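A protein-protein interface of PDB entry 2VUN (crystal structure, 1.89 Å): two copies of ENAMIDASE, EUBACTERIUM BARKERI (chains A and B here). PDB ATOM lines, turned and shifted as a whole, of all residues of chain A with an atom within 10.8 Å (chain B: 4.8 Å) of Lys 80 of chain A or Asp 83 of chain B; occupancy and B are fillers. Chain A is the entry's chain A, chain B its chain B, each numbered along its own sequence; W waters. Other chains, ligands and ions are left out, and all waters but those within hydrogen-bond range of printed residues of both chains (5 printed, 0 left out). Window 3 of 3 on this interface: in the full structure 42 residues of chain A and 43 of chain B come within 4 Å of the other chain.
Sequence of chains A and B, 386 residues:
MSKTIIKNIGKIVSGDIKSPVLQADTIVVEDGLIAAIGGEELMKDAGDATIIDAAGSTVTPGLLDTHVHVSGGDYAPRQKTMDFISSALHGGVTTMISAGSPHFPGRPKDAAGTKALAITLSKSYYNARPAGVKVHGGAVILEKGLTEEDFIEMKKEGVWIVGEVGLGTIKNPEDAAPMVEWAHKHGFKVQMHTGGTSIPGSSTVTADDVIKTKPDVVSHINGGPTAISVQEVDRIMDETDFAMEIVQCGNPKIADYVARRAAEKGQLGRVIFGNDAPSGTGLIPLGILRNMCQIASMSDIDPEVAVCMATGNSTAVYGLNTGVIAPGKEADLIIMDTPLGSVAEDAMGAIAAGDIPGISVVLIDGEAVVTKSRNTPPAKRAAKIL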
ATOM      1  N   HIS A  69       5.575 -27.226   9.022  1.00  0.00           N
ATOM      2  CA  HIS A  69       5.149 -26.973   7.660  1.00  0.00           C
ATOM      3  C   HIS A  69       6.212 -26.148   6.940  1.00  0.00           C
ATOM      4  O   HIS A  69       6.075 -24.937   6.766  1.00  0.00           O
ATOM      5  CB  HIS A  69       3.770 -26.314   7.632  1.00  0.00           C
ATOM      6  CG  HIS A  69       2.663 -27.245   8.008  1.00  0.00           C
ATOM      7  ND1 HIS A  69       2.384 -28.392   7.296  1.00  0.00           N
ATOM      8  CD2 HIS A  69       1.765 -27.203   9.023  1.00  0.00           C
ATOM      9  CE1 HIS A  69       1.359 -29.016   7.854  1.00  0.00           C
ATOM     10  NE2 HIS A  69       0.967 -28.317   8.905  1.00  0.00           N
ATOM     11  N   SER A  71       8.704 -25.115   3.682  1.00  0.00           N
ATOM     12  CA  SER A  71       8.397 -24.801   2.293  1.00  0.00           C
ATOM     13  C   SER A  71       9.660 -24.492   1.487  1.00  0.00           C
ATOM     14  O   SER A  71       9.578 -23.974   0.372  1.00  0.00           O
ATOM     15  CB  SER A  71       7.355 -23.662   2.202  1.00  0.00           C
ATOM     16  OG  SER A  71       7.745 -22.538   2.976  1.00  0.00           O
ATOM     17  N   ASP A  74      14.783 -21.587   5.093  1.00  0.00           N
ATOM     18  CA  ASP A  74      14.449 -21.185   6.461  1.00  0.00           C
ATOM     19  C   ASP A  74      13.497 -19.971   6.507  1.00  0.00           C
ATOM     20  O   ASP A  74      13.453 -19.234   7.496  1.00  0.00           O
ATOM     21  CB  ASP A  74      15.744 -20.942   7.267  1.00  0.00           C
ATOM     22  CG  ASP A  74      15.526 -20.991   8.780  1.00  0.00           C
ATOM     23  OD1 ASP A  74      14.350 -21.038   9.203  1.00  0.00           O
ATOM     24  OD2 ASP A  74      16.522 -20.969   9.561  1.00  0.00           O
ATOM     25  N   TYR A  75      12.721 -19.779   5.447  1.00  0.00           N
ATOM     26  CA  TYR A  75      11.701 -18.734   5.424  1.00  0.00           C
ATOM     27  C   TYR A  75      10.302 -19.354   5.517  1.00  0.00           C
ATOM     28  O   TYR A  75      10.020 -20.361   4.858  1.00  0.00           O
ATOM     29  CB  TYR A  75      11.840 -17.880   4.156  1.00  0.00           C
ATOM     30  CG  TYR A  75      10.744 -16.848   4.004  1.00  0.00           C
ATOM     31  CD1 TYR A  75      10.651 -15.772   4.883  1.00  0.00           C
ATOM     32  CD2 TYR A  75       9.795 -16.958   2.986  1.00  0.00           C
ATOM     33  CE1 TYR A  75       9.631 -14.828   4.756  1.00  0.00           C
ATOM     34  CE2 TYR A  75       8.776 -16.023   2.851  1.00  0.00           C
ATOM     35  CZ  TYR A  75       8.703 -14.961   3.740  1.00  0.00           C
ATOM     36  OH  TYR A  75       7.696 -14.029   3.606  1.00  0.00           O
ATOM     37  N   ALA A  76       9.439 -18.763   6.341  1.00  0.00           N
ATOM     38  CA  ALA A  76       8.057 -19.221   6.474  1.00  0.00           C
ATOM     39  C   ALA A  76       7.065 -18.170   5.957  1.00  0.00           C
ATOM     40  O   ALA A  76       6.786 -17.178   6.646  1.00  0.00           O
ATOM     41  CB  ALA A  76       7.752 -19.603   7.934  1.00  0.00           C
ATOM     42  N   PRO A  77       6.523 -18.384   4.739  1.00  0.00           N
ATOM     43  CA  PRO A  77       5.566 -17.446   4.138  1.00  0.00           C
ATOM     44  C   PRO A  77       4.302 -17.239   4.978  1.00  0.00           C
ATOM     45  O   PRO A  77       3.776 -16.121   5.032  1.00  0.00           O
ATOM     46  CB  PRO A  77       5.181 -18.114   2.806  1.00  0.00           C
ATOM     47  CG  PRO A  77       6.230 -19.124   2.535  1.00  0.00           C
ATOM     48  CD  PRO A  77       6.786 -19.547   3.869  1.00  0.00           C
ATOM     49  N   ARG A  78       3.824 -18.299   5.632  1.00  0.00           N
ATOM     50  CA  ARG A  78       2.548 -18.236   6.367  1.00  0.00           C
ATOM     51  C   ARG A  78       2.520 -17.119   7.417  1.00  0.00           C
ATOM     52  O   ARG A  78       1.475 -16.508   7.643  1.00  0.00           O
ATOM     53  CB  ARG A  78       2.225 -19.577   7.031  1.00  0.00           C
ATOM     54  CG  ARG A  78       0.836 -19.673   7.667  1.00  0.00           C
ATOM     55  CD  ARG A  78      -0.299 -19.425   6.663  1.00  0.00           C
ATOM     56  NE  ARG A  78      -1.616 -19.736   7.228  1.00  0.00           N
ATOM     57  CZ  ARG A  78      -2.367 -18.868   7.908  1.00  0.00           C
ATOM     58  NH1 ARG A  78      -1.933 -17.633   8.129  1.00  0.00           N
ATOM     59  NH2 ARG A  78      -3.555 -19.243   8.382  1.00  0.00           N
ATOM     60  N   GLN A  79       3.656 -16.871   8.062  1.00  0.00           N
ATOM     61  CA  GLN A  79       3.753 -15.792   9.042  1.00  0.00           C
ATOM     62  C   GLN A  79       4.885 -14.807   8.724  1.00  0.00           C
ATOM     63  O   GLN A  79       5.308 -14.062   9.600  1.00  0.00           O
ATOM     64  CB  GLN A  79       3.891 -16.347  10.473  1.00  0.00           C
ATOM     65  CG  GLN A  79       2.659 -17.093  11.004  1.00  0.00           C
ATOM     66  CD  GLN A  79       1.441 -16.199  11.229  1.00  0.00           C
ATOM     67  OE1 GLN A  79       1.533 -14.966  11.190  1.00  0.00           O
ATOM     68  NE2 GLN A  79       0.286 -16.824  11.462  1.00  0.00           N
ATOM     69  N   LYS A  80       5.354 -14.806   7.476  1.00  0.00           N
ATOM     70  CA  LYS A  80       6.414 -13.886   7.015  1.00  0.00           C
ATOM     71  C   LYS A  80       7.614 -13.854   7.969  1.00  0.00           C
ATOM     72  O   LYS A  80       8.059 -12.781   8.397  1.00  0.00           O
ATOM     73  CB  LYS A  80       5.846 -12.473   6.802  1.00  0.00           C
ATOM     74  CG  LYS A  80       4.664 -12.434   5.847  1.00  0.00           C
ATOM     75  CD  LYS A  80       4.155 -11.010   5.643  1.00  0.00           C
ATOM     76  CE  LYS A  80       2.759 -11.008   5.025  1.00  0.00           C
ATOM     77  NZ  LYS A  80       2.761 -11.470   3.608  1.00  0.00           N
ATOM     78  N   THR A  81       8.123 -15.039   8.307  1.00  0.00           N
ATOM     79  CA  THR A  81       9.179 -15.164   9.302  1.00  0.00           C
ATOM     80  C   THR A  81      10.450 -15.729   8.690  1.00  0.00           C
ATOM     81  O   THR A  81      10.427 -16.790   8.054  1.00  0.00           O
ATOM     82  CB  THR A  81       8.741 -16.094  10.462  1.00  0.00           C
ATOM     83  OG1 THR A  81       7.481 -15.653  10.982  1.00  0.00           O
ATOM     84  CG2 THR A  81       9.781 -16.111  11.580  1.00  0.00           C
ATOM     85  N   MET A  82      11.555 -15.015   8.887  1.00  0.00           N
ATOM     86  CA  MET A  82      12.854 -15.467   8.418  1.00  0.00           C
ATOM     87  C   MET A  82      13.564 -16.215   9.549  1.00  0.00           C
ATOM     88  O   MET A  82      13.355 -15.912  10.728  1.00  0.00           O
ATOM     89  CB  MET A  82      13.694 -14.279   7.912  1.00  0.00           C
ATOM     90  CG  MET A  82      13.015 -13.477   6.766  1.00  0.00           C
ATOM     91  SD  MET A  82      13.834 -11.946   6.212  1.00  0.00           S
ATOM     92  CE  MET A  82      13.369 -10.796   7.520  1.00  0.00           C
ATOM     93  N   ASP A  83      14.378 -17.204   9.180  1.00  0.00           N
ATOM     94  CA  ASP A  83      15.263 -17.911  10.119  1.00  0.00           C
ATOM     95  C   ASP A  83      14.530 -18.656  11.233  1.00  0.00           C
ATOM     96  O   ASP A  83      15.020 -18.717  12.370  1.00  0.00           O
ATOM     97  CB  ASP A  83      16.281 -16.948  10.747  1.00  0.00           C
ATOM     98  CG  ASP A  83      17.445 -16.624   9.827  1.00  0.00           C
ATOM     99  OD1 ASP A  83      17.649 -17.334   8.815  1.00  0.00           O
ATOM    100  OD2 ASP A  83      18.175 -15.653  10.137  1.00  0.00           O
ATOM    101  N   PHE A  84      13.368 -19.225  10.928  1.00  0.00           N
ATOM    102  CA  PHE A  84      12.585 -19.892  11.975  1.00  0.00           C
ATOM    103  C   PHE A  84      13.161 -21.236  12.433  1.00  0.00           C
ATOM    104  O   PHE A  84      12.917 -21.670  13.562  1.00  0.00           O
ATOM    105  CB  PHE A  84      11.113 -20.032  11.569  1.00  0.00           C
ATOM    106  CG  PHE A  84      10.835 -21.149  10.597  1.00  0.00           C
ATOM    107  CD1 PHE A  84      10.426 -22.400  11.059  1.00  0.00           C
ATOM    108  CD2 PHE A  84      10.934 -20.945   9.232  1.00  0.00           C
ATOM    109  CE1 PHE A  84      10.140 -23.438  10.163  1.00  0.00           C
ATOM    110  CE2 PHE A  84      10.655 -21.981   8.325  1.00  0.00           C
ATOM    111  CZ  PHE A  84      10.258 -23.221   8.794  1.00  0.00           C
ATOM    112  N   HIS A 103       1.930 -24.253   2.334  1.00  0.00           N
ATOM    113  CA  HIS A 103       2.197 -22.823   2.148  1.00  0.00           C
ATOM    114  C   HIS A 103       3.157 -22.522   0.997  1.00  0.00           C
ATOM    115  O   HIS A 103       3.513 -21.359   0.770  1.00  0.00           O
ATOM    116  CB  HIS A 103       2.736 -22.205   3.443  1.00  0.00           C
ATOM    117  CG  HIS A 103       1.949 -22.575   4.665  1.00  0.00           C
ATOM    118  ND1 HIS A 103       2.546 -23.012   5.826  1.00  0.00           N
ATOM    119  CD2 HIS A 103       0.615 -22.575   4.903  1.00  0.00           C
ATOM    120  CE1 HIS A 103       1.613 -23.278   6.725  1.00  0.00           C
ATOM    121  NE2 HIS A 103       0.434 -23.014   6.193  1.00  0.00           N
ATOM    122  N   PRO A 105       4.240 -21.282  -2.242  1.00  0.00           N
ATOM    123  CA  PRO A 105       3.490 -20.349  -3.095  1.00  0.00           C
ATOM    124  C   PRO A 105       3.120 -21.019  -4.413  1.00  0.00           C
ATOM    125  O   PRO A 105       3.991 -21.572  -5.076  1.00  0.00           O
ATOM    126  CB  PRO A 105       4.466 -19.185  -3.313  1.00  0.00           C
ATOM    127  CG  PRO A 105       5.816 -19.721  -2.925  1.00  0.00           C
ATOM    128  CD  PRO A 105       5.591 -20.792  -1.913  1.00  0.00           C
ATOM    129  N   ALA A 277       3.233 -25.709  13.175  1.00  0.00           N
ATOM    130  CA  ALA A 277       3.559 -24.359  12.767  1.00  0.00           C
ATOM    131  C   ALA A 277       4.658 -24.471  11.715  1.00  0.00           C
ATOM    132  O   ALA A 277       5.342 -25.494  11.658  1.00  0.00           O
ATOM    133  CB  ALA A 277       4.023 -23.522  13.970  1.00  0.00           C
ATOM    134  N   PRO A 278       4.823 -23.437  10.866  1.00  0.00           N
ATOM    135  CA  PRO A 278       3.996 -22.232  10.768  1.00  0.00           C
ATOM    136  C   PRO A 278       2.535 -22.556  10.510  1.00  0.00           C
ATOM    137  O   PRO A 278       2.213 -23.520   9.796  1.00  0.00           O
ATOM    138  CB  PRO A 278       4.594 -21.468   9.572  1.00  0.00           C
ATOM    139  CG  PRO A 278       5.568 -22.385   8.944  1.00  0.00           C
ATOM    140  CD  PRO A 278       5.973 -23.399   9.950  1.00  0.00           C
ATOM    141  N   SER A 279       1.667 -21.750  11.113  1.00  0.00           N
ATOM    142  CA  SER A 279       0.228 -21.918  11.019  1.00  0.00           C
ATOM    143  C   SER A 279      -0.401 -20.574  11.344  1.00  0.00           C
ATOM    144  O   SER A 279       0.315 -19.604  11.636  1.00  0.00           O
ATOM    145  CB  SER A 279      -0.250 -22.963  12.035  1.00  0.00           C
ATOM    146  OG  SER A 279       0.100 -22.574  13.366  1.00  0.00           O
ATOM    147  N   GLY A 280      -1.733 -20.516  11.307  1.00  0.00           N
ATOM    148  CA  GLY A 280      -2.458 -19.286  11.660  1.00  0.00           C
ATOM    149  C   GLY A 280      -2.154 -18.838  13.079  1.00  0.00           C
ATOM    150  O   GLY A 280      -2.169 -17.643  13.377  1.00  0.00           O
ATOM    151  N   THR A 281      -1.889 -19.805  13.962  1.00  0.00           N
ATOM    152  CA  THR A 281      -1.548 -19.520  15.362  1.00  0.00           C
ATOM    153  C   THR A 281      -0.281 -18.676  15.531  1.00  0.00           C
ATOM    154  O   THR A 281      -0.247 -17.740  16.353  1.00  0.00           O
ATOM    155  CB  THR A 281      -1.426 -20.828  16.181  1.00  0.00           C
ATOM    156  OG1 THR A 281      -2.706 -21.460  16.231  1.00  0.00           O
ATOM    157  CG2 THR A 281      -0.956 -20.550  17.617  1.00  0.00           C
ATOM    158  N   GLY A 282       0.749 -19.009  14.762  1.00  0.00           N
ATOM    159  CA  GLY A 282       2.018 -18.294  14.820  1.00  0.00           C
ATOM    160  C   GLY A 282       3.205 -19.176  14.506  1.00  0.00           C
ATOM    161  O   GLY A 282       3.104 -20.127  13.735  1.00  0.00           O
ATOM    162  N   LEU A 283       4.336 -18.834  15.104  1.00  0.00           N
ATOM    163  CA  LEU A 283       5.560 -19.603  14.976  1.00  0.00           C
ATOM    164  C   LEU A 283       6.213 -19.541  16.352  1.00  0.00           C
ATOM    165  O   LEU A 283       6.451 -18.452  16.901  1.00  0.00           O
ATOM    166  CB  LEU A 283       6.438 -18.998  13.878  1.00  0.00           C
ATOM    167  CG  LEU A 283       7.425 -19.780  13.006  1.00  0.00           C
ATOM    168  CD1 LEU A 283       7.211 -21.305  12.928  1.00  0.00           C
ATOM    169  CD2 LEU A 283       7.411 -19.154  11.621  1.00  0.00           C
ATOM    170  N   ASP B  74       5.783  -2.414  11.793  1.00  0.00           N
ATOM    171  CA  ASP B  74       5.236  -3.761  11.951  1.00  0.00           C
ATOM    172  C   ASP B  74       6.267  -4.876  11.754  1.00  0.00           C
ATOM    173  O   ASP B  74       5.912  -6.016  11.424  1.00  0.00           O
ATOM    174  CB  ASP B  74       4.040  -3.948  11.017  1.00  0.00           C
ATOM    175  CG  ASP B  74       4.336  -3.512   9.593  1.00  0.00           C
ATOM    176  OD1 ASP B  74       5.521  -3.521   9.171  1.00  0.00           O
ATOM    177  OD2 ASP B  74       3.378  -3.140   8.885  1.00  0.00           O
ATOM    178  N   LYS B  80      12.631 -11.901  13.672  1.00  0.00           N
ATOM    179  CA  LYS B  80      12.701 -11.609  12.234  1.00  0.00           C
ATOM    180  C   LYS B  80      11.348 -11.840  11.536  1.00  0.00           C
ATOM    181  O   LYS B  80      11.243 -12.592  10.561  1.00  0.00           O
ATOM    182  CB  LYS B  80      13.822 -12.436  11.583  1.00  0.00           C
ATOM    183  CG  LYS B  80      15.197 -12.245  12.232  1.00  0.00           C
ATOM    184  CD  LYS B  80      16.255 -13.088  11.523  1.00  0.00           C
ATOM    185  CE  LYS B  80      17.671 -12.663  11.915  1.00  0.00           C
ATOM    186  NZ  LYS B  80      18.103 -13.402  13.131  1.00  0.00           N
ATOM    187  N   THR B  81      10.310 -11.185  12.054  1.00  0.00           N
ATOM    188  CA  THR B  81       8.955 -11.373  11.563  1.00  0.00           C
ATOM    189  C   THR B  81       8.400 -10.062  11.023  1.00  0.00           C
ATOM    190  O   THR B  81       8.427  -9.035  11.705  1.00  0.00           O
ATOM    191  CB  THR B  81       8.023 -11.889  12.691  1.00  0.00           C
ATOM    192  OG1 THR B  81       8.576 -13.079  13.272  1.00  0.00           O
ATOM    193  CG2 THR B  81       6.610 -12.169  12.170  1.00  0.00           C
ATOM    194  N   MET B  82       7.896 -10.107   9.798  1.00  0.00           N
ATOM    195  CA  MET B  82       7.279  -8.947   9.173  1.00  0.00           C
ATOM    196  C   MET B  82       5.762  -9.025   9.363  1.00  0.00           C
ATOM    197  O   MET B  82       5.197 -10.120   9.490  1.00  0.00           O
ATOM    198  CB  MET B  82       7.653  -8.887   7.683  1.00  0.00           C
ATOM    199  CG  MET B  82       9.183  -8.907   7.430  1.00  0.00           C
ATOM    200  SD  MET B  82       9.737  -8.804   5.704  1.00  0.00           S
ATOM    201  CE  MET B  82       9.692 -10.525   5.168  1.00  0.00           C
ATOM    202  N   ASP B  83       5.118  -7.862   9.399  1.00  0.00           N
ATOM    203  CA  ASP B  83       3.646  -7.749   9.459  1.00  0.00           C
ATOM    204  C   ASP B  83       2.995  -8.462  10.639  1.00  0.00           C
ATOM    205  O   ASP B  83       1.893  -9.012  10.492  1.00  0.00           O
ATOM    206  CB  ASP B  83       3.003  -8.262   8.161  1.00  0.00           C
ATOM    207  CG  ASP B  83       3.213  -7.328   6.993  1.00  0.00           C
ATOM    208  OD1 ASP B  83       3.524  -6.135   7.221  1.00  0.00           O
ATOM    209  OD2 ASP B  83       3.058  -7.790   5.838  1.00  0.00           O
ATOM    210  N   PHE B  84       3.649  -8.459  11.801  1.00  0.00           N
ATOM    211  CA  PHE B  84       3.115  -9.203  12.953  1.00  0.00           C
ATOM    212  C   PHE B  84       1.877  -8.548  13.580  1.00  0.00           C
ATOM    213  O   PHE B  84       1.064  -9.219  14.226  1.00  0.00           O
ATOM    214  CB  PHE B  84       4.199  -9.480  14.003  1.00  0.00           C
ATOM    215  CG  PHE B  84       4.522  -8.305  14.891  1.00  0.00           C
ATOM    216  CD1 PHE B  84       3.906  -8.162  16.128  1.00  0.00           C
ATOM    217  CD2 PHE B  84       5.464  -7.353  14.497  1.00  0.00           C
ATOM    218  CE1 PHE B  84       4.204  -7.067  16.964  1.00  0.00           C
ATOM    219  CE2 PHE B  84       5.768  -6.261  15.316  1.00  0.00           C
ATOM    220  CZ  PHE B  84       5.139  -6.116  16.549  1.00  0.00           C
ATOM    221  N   ILE B  85       1.734  -7.245  13.379  1.00  0.00           N
ATOM    222  CA  ILE B  85       0.599  -6.523  13.958  1.00  0.00           C
ATOM    223  C   ILE B  85      -0.683  -6.787  13.167  1.00  0.00           C
ATOM    224  O   ILE B  85      -1.738  -7.072  13.749  1.00  0.00           O
ATOM    225  CB  ILE B  85       0.903  -5.008  14.128  1.00  0.00           C
ATOM    226  CG1 ILE B  85       2.013  -4.817  15.173  1.00  0.00           C
ATOM    227  CG2 ILE B  85      -0.354  -4.266  14.538  1.00  0.00           C
ATOM    228  CD1 ILE B  85       2.631  -3.410  15.246  1.00  0.00           C
ATOM    229  N   SER B  86      -0.597  -6.727  11.840  1.00  0.00           N
ATOM    230  CA  SER B  86      -1.744  -7.112  11.028  1.00  0.00           C
ATOM    231  C   SER B  86      -2.109  -8.582  11.282  1.00  0.00           C
ATOM    232  O   SER B  86      -3.280  -8.941  11.286  1.00  0.00           O
ATOM    233  CB  SER B  86      -1.523  -6.811   9.538  1.00  0.00           C
ATOM    234  OG  SER B  86      -0.938  -7.895   8.854  1.00  0.00           O
ATOM    235  N   SER B  87      -1.108  -9.425  11.532  1.00  0.00           N
ATOM    236  CA  SER B  87      -1.385 -10.825  11.873  1.00  0.00           C
ATOM    237  C   SER B  87      -2.173 -10.950  13.186  1.00  0.00           C
ATOM    238  O   SER B  87      -3.157 -11.701  13.248  1.00  0.00           O
ATOM    239  CB  SER B  87      -0.102 -11.647  11.918  1.00  0.00           C
ATOM    240  OG  SER B  87      -0.389 -13.024  11.729  1.00  0.00           O
ATOM    241  N   ARG B 374      -7.616 -14.401   8.394  1.00  0.00           N
ATOM    242  CA  ARG B 374      -6.641 -15.230   7.684  1.00  0.00           C
ATOM    243  C   ARG B 374      -5.904 -16.181   8.628  1.00  0.00           C
ATOM    244  O   ARG B 374      -5.162 -17.049   8.173  1.00  0.00           O
ATOM    245  CB  ARG B 374      -5.636 -14.353   6.911  1.00  0.00           C
ATOM    246  CG  ARG B 374      -4.520 -13.747   7.760  1.00  0.00           C
ATOM    247  CD  ARG B 374      -3.563 -12.910   6.893  1.00  0.00           C
ATOM    248  NE  ARG B 374      -2.384 -12.439   7.624  1.00  0.00           N
ATOM    249  CZ  ARG B 374      -2.081 -11.158   7.825  1.00  0.00           C
ATOM    250  NH1 ARG B 374      -2.855 -10.197   7.341  1.00  0.00           N
ATOM    251  NH2 ARG B 374      -0.975 -10.835   8.487  1.00  0.00           N
HETATM  252  O   HOH W   1       3.591 -12.165  10.754  1.00  0.00           O
HETATM  253  O   HOH W   2       1.440 -12.769   8.770  1.00  0.00           O
HETATM  254  O   HOH W   3      -6.872 -19.686   8.464  1.00  0.00           O
HETATM  255  O   HOH W   4       7.019 -15.365  13.786  1.00  0.00           O
HETATM  256  O   HOH W   5      -0.940 -14.596   8.840  1.00  0.00           O
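The side-chain amide oxygen (OE1) of Gln 79 of chain A lies within hydrogen-bond range of the side-chain hydroxyl (OG) of Ser 87 of chain B, at 2.8 Å. The backbone NH (N) of Met 82 of chain A sits at hydrogen-bond distance from the backbone carbonyl oxygen (O) of Lys 80 of chain B, at 3.0 Å. The backbone carbonyl oxygen of Lys 80 of chain A sits at hydrogen-bond distance from the backbone NH of Met 82 of chain B (3.0 Å). The backbone carbonyl oxygen (O) of Arg 374 of chain B sits at hydrogen-bond distance from the guanidinium group (NH2) of Arg 78 of chain A (2.7 Å). The side-chain carboxylate (OD2) of Asp 83 of chain A lies within salt-bridge range of the side-chain amino group (NZ) of Lys 80 of chain B (3.7 Å).
The backbone carbonyl oxygen (O) of Asp 74 of chain B is in hydrogen-bond range of the backbone NH (N) of Asp 83 of chain B (2.9 Å). The backbone NH (N) of Ala 76 of chain A is in hydrogen-bond range of the backbone carbonyl oxygen (O) of Thr 81 of chain A (2.8 Å). The backbone carbonyl oxygen (O) of Gln 79 of chain A lies within hydrogen-bond range of the side-chain hydroxyl (OG1) of Thr 81 of chain A (3.0 Å). The backbone carbonyl oxygen (O) of Asp 83 of chain B is in hydrogen-bond range of the side-chain hydroxyl (OG) of Ser 86 of chain B, at 3.5 Å. O of Asp 74 of chain A is in hydrogen-bond range of N of Asp 83 of chain A, at 2.8 Å. The side-chain amide nitrogen of Gln 79 of chain A lies within hydrogen-bond range of the backbone carbonyl oxygen of Gly 280 of chain A, 3.2 Å away.
Among the printed residues, pairs that only touch across the chains: Lys 80 of chain A with Asp 83 of chain B (3.3 Å), Gln 79 of chain A with Thr 81 of chain B (3.4 Å), Thr 81 of chain A with Lys 80 of chain B (3.5 Å), Lys 80 of chain A with Thr 81 of chain B (3.6 Å), Thr 81 of chain A with Thr 81 of chain B (3.6 Å), Lys 80 of chain A with Lys 80 of chain B (3.9 Å) and Gln 79 of chain A with Met 82 of chain B (3.9 Å).
Of the printed residues of chain B, Lys 80 of chain A touches Lys 80, Thr 81, Met 82 and Asp 83. Asp 83 of chain B touches just one residue of chain A: Lys 80. No residue of chain A comes within 4 Å of Asp 74 of chain B. Met 82 of chain B touches just these residues of chain A: Gln 79 and Lys 80. No residue of chain A comes within 4 Å of Ser 86 of chain B. Of the printed residues of chain A, Ser 87 of chain B touches Gln 79. Printed residues of chain B within 4 Å of Asp 83 of chain A: Lys 80. Of the printed residues of chain B, Thr 81 of chain A touches Lys 80 (3.5 Å) and Thr 81 (3.6 Å). Printed residues of chain A within 4 Å of Lys 80 of chain B: Lys 80 (3.9 Å), Thr 81 (3.5 Å), Met 82 (3.0 Å) and Asp 83 (3.5 Å). Ala 76 of chain A touches none of the printed residues of chain B. Pro 105 of chain A touches none of the printed residues of chain B. The nearest residue of chain A that does not touch Asp 83 of chain B is Gln 79 of chain A (6.0 Å).
Printed residues of chain B that touch a printed residue of chain A: Lys 80, Thr 81, Met 82, Asp 83, Ser 87 and Arg 374. Hydrophobic or aromatic side chains of chain B within 4 Å of the printed part of chain A: Met 82.
Lys 80 of chain B touches its own counterpart, Lys 80 of chain A. Lys 80 of chain A touches Thr 81 of chain B, and with the chains exchanged Thr 81 of chain A touches Lys 80 of chain B. Lys 80 of chain A touches Met 82 of chain B, and with the chains exchanged Met 82 of chain A touches Lys 80 of chain B. Thr 81 of chain A touches its own counterpart, Thr 81 of chain B.
Water W1 bridges the backbone carbonyl oxygen of Gln 79 of chain A (2.8 Å) and the backbone carbonyl oxygen of Met 82 of chain B (2.9 Å). Water W4 lies within hydrogen-bond range of the side-chain hydroxyl (OG1) of Thr 81 of chain B (2.8 Å) and the side-chain hydroxyl (OG1) of Thr 81 of chain A (2.9 Å). Water W5 lies within hydrogen-bond range of NE of Arg 374 of chain B (2.9 Å), NH1 of Arg 78 of chain A (3.3 Å), OG of Ser 87 of chain B (3.3 Å) and OE1 of Gln 79 of chain A (3.4 Å). Water W2 lies within hydrogen-bond range of NH2 of Arg 374 of chain B, OE1 of Gln 79 of chain A and OG of Ser 87 of chain B. Water W3 bridges O of Arg 374 of chain B (3.2 Å) and NH2 of Arg 78 of chain A (3.3 Å).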
